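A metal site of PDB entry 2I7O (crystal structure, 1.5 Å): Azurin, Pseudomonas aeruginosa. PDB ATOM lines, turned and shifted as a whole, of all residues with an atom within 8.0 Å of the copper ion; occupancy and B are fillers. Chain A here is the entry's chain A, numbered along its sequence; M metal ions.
Residues that only touch the copper ion: Gly 45, Phe 114 and Met 121.
Within 4 Å of the copper ion: Gly 45, His 46, Cys 112, Phe 114, His 117 and Met 121.
The nearest printed residue that does not touch the copper ion is Asn 47 (4.5 Å).
A ring nitrogen (NE2) of His 46 lies within hydrogen-bond range of the backbone carbonyl oxygen (O) of Asn 10 (2.8 Å).
SD of Met 121 lies close to ND1 of His 46 (3.3 Å).
SG of Cys 112 lies close to N of Asn 47 (3.5 Å).
NE2 of His 117 sits close to SD of Met 44.
The backbone NH (N) of Phe 114 sits close to the side-chain sulfur (SG) of Cys 112 (3.4 Å).
A ring nitrogen (ND1) of His 117 lies close to the side-chain sulfur (SD) of Met 121, 3.8 Å away.
The backbone NH (N) of Ile 87 sits at hydrogen-bond distance from the backbone carbonyl oxygen (O) of His 46 (2.8 Å).
O of Gly 45 sits close to ND1 of His 117, at 3.4 Å.
The copper ion is bound by ND1 of His 46 (2.0 Å), ND1 of His 117 (2.0 Å) and SG of Cys 112 (2.2 Å).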
ATOM      1  N   GLY A   9      -5.963 -23.337   2.297  1.00  0.00           N
ATOM      2  CA  GLY A   9      -6.595 -23.752   1.053  1.00  0.00           C
ATOM      3  C   GLY A   9      -7.835 -24.523   1.485  1.00  0.00           C
ATOM      4  O   GLY A   9      -7.721 -25.476   2.250  1.00  0.00           O
ATOM      5  N   ASN A  10      -9.022 -24.132   1.012  1.00  0.00           N
ATOM      6  CA  ASN A  10     -10.260 -24.788   1.436  1.00  0.00           C
ATOM      7  C   ASN A  10     -10.969 -25.672   0.416  1.00  0.00           C
ATOM      8  O   ASN A  10     -10.442 -25.941  -0.662  1.00  0.00           O
ATOM      9  CB  ASN A  10     -11.253 -23.731   1.959  1.00  0.00           C
ATOM     10  CG  ASN A  10     -11.665 -22.738   0.890  1.00  0.00           C
ATOM     11  OD1 ASN A  10     -11.490 -22.983  -0.289  1.00  0.00           O
ATOM     12  ND2 ASN A  10     -12.239 -21.619   1.317  1.00  0.00           N
ATOM     13  N   MET A  13     -11.772 -24.489  -3.360  1.00  0.00           N
ATOM     14  CA  MET A  13     -10.656 -24.293  -4.275  1.00  0.00           C
ATOM     15  C   MET A  13     -10.135 -22.842  -4.228  1.00  0.00           C
ATOM     16  O   MET A  13      -9.927 -22.203  -5.259  1.00  0.00           O
ATOM     17  CB  MET A  13     -11.098 -24.654  -5.709  1.00  0.00           C
ATOM     18  CG  MET A  13      -9.964 -25.019  -6.649  1.00  0.00           C
ATOM     19  SD  MET A  13     -10.562 -25.511  -8.299  1.00  0.00           S
ATOM     20  CE  MET A  13     -10.900 -23.919  -9.045  1.00  0.00           C
ATOM     21  N   GLN A  14      -9.901 -22.344  -3.023  1.00  0.00           N
ATOM     22  CA  GLN A  14      -9.416 -20.986  -2.839  1.00  0.00           C
ATOM     23  C   GLN A  14      -8.383 -20.883  -1.720  1.00  0.00           C
ATOM     24  O   GLN A  14      -8.464 -21.610  -0.726  1.00  0.00           O
ATOM     25  CB  GLN A  14     -10.585 -20.054  -2.482  1.00  0.00           C
ATOM     26  CG  GLN A  14     -11.407 -19.532  -3.650  1.00  0.00           C
ATOM     27  CD  GLN A  14     -11.067 -18.098  -4.031  1.00  0.00           C
ATOM     28  OE1 GLN A  14     -11.754 -17.482  -4.844  1.00  0.00           O
ATOM     29  NE2 GLN A  14      -9.999 -17.570  -3.431  1.00  0.00           N
ATOM     30  N   PHE A  15      -7.410 -19.990  -1.900  1.00  0.00           N
ATOM     31  CA  PHE A  15      -6.412 -19.703  -0.858  1.00  0.00           C
ATOM     32  C   PHE A  15      -7.048 -18.520  -0.117  1.00  0.00           C
ATOM     33  O   PHE A  15      -7.925 -17.854  -0.660  1.00  0.00           O
ATOM     34  CB  PHE A  15      -5.084 -19.226  -1.448  1.00  0.00           C
ATOM     35  CG  PHE A  15      -4.161 -20.320  -1.909  1.00  0.00           C
ATOM     36  CD1 PHE A  15      -3.857 -21.400  -1.090  1.00  0.00           C
ATOM     37  CD2 PHE A  15      -3.560 -20.233  -3.172  1.00  0.00           C
ATOM     38  CE1 PHE A  15      -2.943 -22.382  -1.506  1.00  0.00           C
ATOM     39  CE2 PHE A  15      -2.647 -21.209  -3.601  1.00  0.00           C
ATOM     40  CZ  PHE A  15      -2.343 -22.283  -2.763  1.00  0.00           C
ATOM     41  N   LEU A  33       1.172 -23.980   5.457  1.00  0.00           N
ATOM     42  CA  LEU A  33      -0.061 -24.312   4.759  1.00  0.00           C
ATOM     43  C   LEU A  33      -0.993 -25.244   5.538  1.00  0.00           C
ATOM     44  O   LEU A  33      -0.543 -26.214   6.156  1.00  0.00           O
ATOM     45  CB  LEU A  33       0.274 -24.988   3.411  1.00  0.00           C
ATOM     46  CG  LEU A  33      -0.925 -25.310   2.520  1.00  0.00           C
ATOM     47  CD1 LEU A  33      -1.534 -24.022   1.994  1.00  0.00           C
ATOM     48  CD2 LEU A  33      -0.475 -26.215   1.374  1.00  0.00           C
ATOM     49  N   HIS A  35      -5.355 -26.856   5.558  1.00  0.00           N
ATOM     50  CA  HIS A  35      -6.479 -27.118   4.671  1.00  0.00           C
ATOM     51  C   HIS A  35      -7.809 -27.231   5.387  1.00  0.00           C
ATOM     52  O   HIS A  35      -8.246 -28.331   5.709  1.00  0.00           O
ATOM     53  CB  HIS A  35      -6.224 -28.425   3.901  1.00  0.00           C
ATOM     54  CG  HIS A  35      -7.201 -28.711   2.796  1.00  0.00           C
ATOM     55  ND1 HIS A  35      -8.552 -28.422   2.882  1.00  0.00           N
ATOM     56  CD2 HIS A  35      -7.034 -29.335   1.602  1.00  0.00           C
ATOM     57  CE1 HIS A  35      -9.166 -28.851   1.803  1.00  0.00           C
ATOM     58  NE2 HIS A  35      -8.270 -29.408   1.003  1.00  0.00           N
ATOM     59  N   LYS A  41      -7.441 -35.475  -0.082  1.00  0.00           N
ATOM     60  CA  LYS A  41      -6.419 -35.094  -1.056  1.00  0.00           C
ATOM     61  C   LYS A  41      -6.757 -35.374  -2.524  1.00  0.00           C
ATOM     62  O   LYS A  41      -6.445 -34.565  -3.397  1.00  0.00           O
ATOM     63  CB  LYS A  41      -5.091 -35.806  -0.740  1.00  0.00           C
ATOM     64  CG  LYS A  41      -4.503 -35.494   0.612  1.00  0.00           C
ATOM     65  CD  LYS A  41      -3.063 -35.034   0.491  1.00  0.00           C
ATOM     66  CE  LYS A  41      -2.213 -36.004  -0.325  1.00  0.00           C
ATOM     67  NZ  LYS A  41      -2.026 -37.322   0.327  1.00  0.00           N
ATOM     68  N   VAL A  43      -9.736 -35.495  -4.052  1.00  0.00           N
ATOM     69  CA  VAL A  43     -10.781 -34.626  -4.589  1.00  0.00           C
ATOM     70  C   VAL A  43     -10.383 -33.158  -4.523  1.00  0.00           C
ATOM     71  O   VAL A  43     -10.669 -32.389  -5.444  1.00  0.00           O
ATOM     72  CB  VAL A  43     -12.107 -34.811  -3.805  1.00  0.00           C
ATOM     73  CG1 VAL A  43     -13.136 -33.794  -4.256  1.00  0.00           C
ATOM     74  CG2 VAL A  43     -12.627 -36.235  -3.989  1.00  0.00           C
ATOM     75  N   MET A  44      -9.725 -32.775  -3.436  1.00  0.00           N
ATOM     76  CA  MET A  44      -9.364 -31.376  -3.230  1.00  0.00           C
ATOM     77  C   MET A  44      -8.008 -31.197  -2.536  1.00  0.00           C
ATOM     78  O   MET A  44      -7.918 -30.482  -1.530  1.00  0.00           O
ATOM     79  CB  MET A  44     -10.471 -30.704  -2.418  1.00  0.00           C
ATOM     80  CG  MET A  44     -10.358 -29.195  -2.295  1.00  0.00           C
ATOM     81  SD  MET A  44     -10.567 -28.343  -3.867  1.00  0.00           S
ATOM     82  CE  MET A  44     -12.354 -28.633  -4.152  1.00  0.00           C
ATOM     83  N   GLY A  45      -6.971 -31.835  -3.056  1.00  0.00           N
ATOM     84  CA  GLY A  45      -5.659 -31.702  -2.453  1.00  0.00           C
ATOM     85  C   GLY A  45      -5.062 -30.354  -2.801  1.00  0.00           C
ATOM     86  O   GLY A  45      -5.304 -29.830  -3.878  1.00  0.00           O
ATOM     87  N   HIS A  46      -4.296 -29.785  -1.870  1.00  0.00           N
ATOM     88  CA  HIS A  46      -3.666 -28.490  -2.103  1.00  0.00           C
ATOM     89  C   HIS A  46      -2.191 -28.456  -1.755  1.00  0.00           C
ATOM     90  O   HIS A  46      -1.756 -29.091  -0.789  1.00  0.00           O
ATOM     91  CB  HIS A  46      -4.318 -27.370  -1.298  1.00  0.00           C
ATOM     92  CG  HIS A  46      -5.758 -27.115  -1.618  1.00  0.00           C
ATOM     93  ND1 HIS A  46      -6.216 -26.958  -2.906  1.00  0.00           N
ATOM     94  CD2 HIS A  46      -6.833 -26.942  -0.810  1.00  0.00           C
ATOM     95  CE1 HIS A  46      -7.514 -26.688  -2.885  1.00  0.00           C
ATOM     96  NE2 HIS A  46      -7.903 -26.671  -1.616  1.00  0.00           N
ATOM     97  N   ASN A  47      -1.422 -27.731  -2.544  1.00  0.00           N
ATOM     98  CA  ASN A  47      -0.019 -27.538  -2.213  1.00  0.00           C
ATOM     99  C   ASN A  47       0.303 -26.065  -2.417  1.00  0.00           C
ATOM    100  O   ASN A  47      -0.533 -25.302  -2.907  1.00  0.00           O
ATOM    101  CB  ASN A  47       0.935 -28.430  -3.040  1.00  0.00           C
ATOM    102  CG  ASN A  47       0.810 -28.243  -4.555  1.00  0.00           C
ATOM    103  OD1 ASN A  47       0.325 -27.236  -5.060  1.00  0.00           O
ATOM    104  ND2 ASN A  47       1.291 -29.248  -5.303  1.00  0.00           N
ATOM    105  N   TRP A  48       1.495 -25.659  -1.980  1.00  0.00           N
ATOM    106  CA  TRP A  48       1.946 -24.286  -2.132  1.00  0.00           C
ATOM    107  C   TRP A  48       3.246 -24.392  -2.921  1.00  0.00           C
ATOM    108  O   TRP A  48       4.216 -24.963  -2.428  1.00  0.00           O
ATOM    109  CB  TRP A  48       2.205 -23.636  -0.777  1.00  0.00           C
ATOM    110  CG  TRP A  48       2.826 -22.272  -0.875  1.00  0.00           C
ATOM    111  CD1 TRP A  48       4.141 -21.983  -1.091  1.00  0.00           C
ATOM    112  CD2 TRP A  48       2.148 -21.028  -0.762  1.00  0.00           C
ATOM    113  NE1 TRP A  48       4.329 -20.622  -1.103  1.00  0.00           N
ATOM    114  CE2 TRP A  48       3.120 -20.014  -0.900  1.00  0.00           C
ATOM    115  CE3 TRP A  48       0.818 -20.665  -0.531  1.00  0.00           C
ATOM    116  CZ2 TRP A  48       2.816 -18.670  -0.825  1.00  0.00           C
ATOM    117  CZ3 TRP A  48       0.514 -19.321  -0.456  1.00  0.00           C
ATOM    118  CH2 TRP A  48       1.509 -18.340  -0.603  1.00  0.00           C
ATOM    119  N   LEU A  86       1.519 -32.082  -1.018  1.00  0.00           N
ATOM    120  CA  LEU A  86       0.099 -31.943  -1.339  1.00  0.00           C
ATOM    121  C   LEU A  86      -0.650 -32.420  -0.095  1.00  0.00           C
ATOM    122  O   LEU A  86      -0.416 -33.531   0.381  1.00  0.00           O
ATOM    123  CB  LEU A  86      -0.275 -32.821  -2.535  1.00  0.00           C
ATOM    124  CG  LEU A  86      -1.666 -32.605  -3.126  1.00  0.00           C
ATOM    125  CD1 LEU A  86      -1.724 -31.255  -3.836  1.00  0.00           C
ATOM    126  CD2 LEU A  86      -1.985 -33.713  -4.111  1.00  0.00           C
ATOM    127  N   ILE A  87      -1.553 -31.590   0.428  1.00  0.00           N
ATOM    128  CA  ILE A  87      -2.289 -31.956   1.623  1.00  0.00           C
ATOM    129  C   ILE A  87      -3.811 -31.968   1.467  1.00  0.00           C
ATOM    130  O   ILE A  87      -4.379 -31.211   0.663  1.00  0.00           O
ATOM    131  CB  ILE A  87      -1.959 -31.030   2.811  1.00  0.00           C
ATOM    132  CG1 ILE A  87      -2.423 -29.602   2.499  1.00  0.00           C
ATOM    133  CG2 ILE A  87      -0.457 -31.059   3.098  1.00  0.00           C
ATOM    134  CD1 ILE A  87      -2.306 -28.647   3.665  1.00  0.00           C
ATOM    135  N   PHE A 111       1.163 -20.763  -6.188  1.00  0.00           N
ATOM    136  CA  PHE A 111      -0.026 -21.415  -6.719  1.00  0.00           C
ATOM    137  C   PHE A 111      -0.075 -22.864  -6.265  1.00  0.00           C
ATOM    138  O   PHE A 111       0.880 -23.387  -5.695  1.00  0.00           O
ATOM    139  CB  PHE A 111       0.022 -21.373  -8.259  1.00  0.00           C
ATOM    140  CG  PHE A 111       1.378 -21.718  -8.834  1.00  0.00           C
ATOM    141  CD1 PHE A 111       2.373 -20.743  -8.936  1.00  0.00           C
ATOM    142  CD2 PHE A 111       1.675 -23.024  -9.220  1.00  0.00           C
ATOM    143  CE1 PHE A 111       3.653 -21.067  -9.374  1.00  0.00           C
ATOM    144  CE2 PHE A 111       2.958 -23.374  -9.670  1.00  0.00           C
ATOM    145  CZ  PHE A 111       3.952 -22.388  -9.744  1.00  0.00           C
ATOM    146  N   CYS A 112      -1.222 -23.494  -6.505  1.00  0.00           N
ATOM    147  CA  CYS A 112      -1.431 -24.908  -6.220  1.00  0.00           C
ATOM    148  C   CYS A 112      -1.374 -25.611  -7.583  1.00  0.00           C
ATOM    149  O   CYS A 112      -1.927 -25.120  -8.568  1.00  0.00           O
ATOM    150  CB  CYS A 112      -2.801 -25.134  -5.572  1.00  0.00           C
ATOM    151  SG  CYS A 112      -3.221 -26.882  -5.372  1.00  0.00           S
ATOM    152  N   THR A 113      -0.705 -26.760  -7.634  1.00  0.00           N
ATOM    153  CA  THR A 113      -0.598 -27.494  -8.888  1.00  0.00           C
ATOM    154  C   THR A 113      -1.593 -28.640  -9.056  1.00  0.00           C
ATOM    155  O   THR A 113      -1.512 -29.372 -10.025  1.00  0.00           O
ATOM    156  CB  THR A 113       0.829 -28.065  -9.094  1.00  0.00           C
ATOM    157  OG1 THR A 113       1.161 -28.948  -8.025  1.00  0.00           O
ATOM    158  CG2 THR A 113       1.840 -26.939  -9.164  1.00  0.00           C
ATOM    159  N   PHE A 114      -2.522 -28.811  -8.108  1.00  0.00           N
ATOM    160  CA  PHE A 114      -3.514 -29.864  -8.286  1.00  0.00           C
ATOM    161  C   PHE A 114      -4.262 -29.493  -9.568  1.00  0.00           C
ATOM    162  O   PHE A 114      -4.575 -28.327  -9.781  1.00  0.00           O
ATOM    163  CB  PHE A 114      -4.480 -29.894  -7.083  1.00  0.00           C
ATOM    164  CG  PHE A 114      -5.489 -31.023  -7.140  1.00  0.00           C
ATOM    165  CD1 PHE A 114      -6.559 -30.969  -8.018  1.00  0.00           C
ATOM    166  CD2 PHE A 114      -5.354 -32.119  -6.302  1.00  0.00           C
ATOM    167  CE1 PHE A 114      -7.505 -32.017  -8.069  1.00  0.00           C
ATOM    168  CE2 PHE A 114      -6.289 -33.175  -6.350  1.00  0.00           C
ATOM    169  CZ  PHE A 114      -7.360 -33.112  -7.231  1.00  0.00           C
ATOM    170  N   PRO A 115      -4.554 -30.470 -10.428  1.00  0.00           N
ATOM    171  CA  PRO A 115      -5.262 -30.215 -11.688  1.00  0.00           C
ATOM    172  C   PRO A 115      -6.411 -29.196 -11.658  1.00  0.00           C
ATOM    173  O   PRO A 115      -7.432 -29.402 -11.000  1.00  0.00           O
ATOM    174  CB  PRO A 115      -5.729 -31.617 -12.089  1.00  0.00           C
ATOM    175  CG  PRO A 115      -4.584 -32.456 -11.642  1.00  0.00           C
ATOM    176  CD  PRO A 115      -4.287 -31.911 -10.259  1.00  0.00           C
ATOM    177  N   GLY A 116      -6.208 -28.095 -12.374  1.00  0.00           N
ATOM    178  CA  GLY A 116      -7.206 -27.040 -12.486  1.00  0.00           C
ATOM    179  C   GLY A 116      -7.267 -25.984 -11.385  1.00  0.00           C
ATOM    180  O   GLY A 116      -7.804 -24.906 -11.589  1.00  0.00           O
ATOM    181  N   HIS A 117      -6.695 -26.274 -10.226  1.00  0.00           N
ATOM    182  CA  HIS A 117      -6.777 -25.324  -9.121  1.00  0.00           C
ATOM    183  C   HIS A 117      -6.143 -23.958  -9.335  1.00  0.00           C
ATOM    184  O   HIS A 117      -6.659 -22.963  -8.819  1.00  0.00           O
ATOM    185  CB  HIS A 117      -6.190 -25.930  -7.838  1.00  0.00           C
ATOM    186  CG  HIS A 117      -6.991 -27.059  -7.280  1.00  0.00           C
ATOM    187  ND1 HIS A 117      -6.772 -27.586  -6.024  1.00  0.00           N
ATOM    188  CD2 HIS A 117      -8.024 -27.780  -7.800  1.00  0.00           C
ATOM    189  CE1 HIS A 117      -7.619 -28.559  -5.798  1.00  0.00           C
ATOM    190  NE2 HIS A 117      -8.389 -28.697  -6.860  1.00  0.00           N
ATOM    191  N   SER A 118      -5.049 -23.897 -10.087  1.00  0.00           N
ATOM    192  CA  SER A 118      -4.368 -22.619 -10.290  1.00  0.00           C
ATOM    193  C   SER A 118      -5.247 -21.552 -10.931  1.00  0.00           C
ATOM    194  O   SER A 118      -4.885 -20.369 -10.915  1.00  0.00           O
ATOM    195  CB  SER A 118      -3.072 -22.806 -11.093  1.00  0.00           C
ATOM    196  OG  SER A 118      -3.326 -23.280 -12.404  1.00  0.00           O
ATOM    197  N   MET A 121      -6.485 -20.565  -7.467  1.00  0.00           N
ATOM    198  CA  MET A 121      -5.457 -20.623  -6.440  1.00  0.00           C
ATOM    199  C   MET A 121      -4.092 -20.144  -6.912  1.00  0.00           C
ATOM    200  O   MET A 121      -3.207 -20.936  -7.236  1.00  0.00           O
ATOM    201  CB  MET A 121      -5.382 -22.031  -5.868  1.00  0.00           C
ATOM    202  CG  MET A 121      -6.712 -22.467  -5.282  1.00  0.00           C
ATOM    203  SD  MET A 121      -6.682 -24.107  -4.514  1.00  0.00           S
ATOM    204  CE  MET A 121      -5.886 -23.696  -2.899  1.00  0.00           C
HETATM  205 CU    CU M   1      -5.302 -27.001  -4.723  1.00  0.00          CU
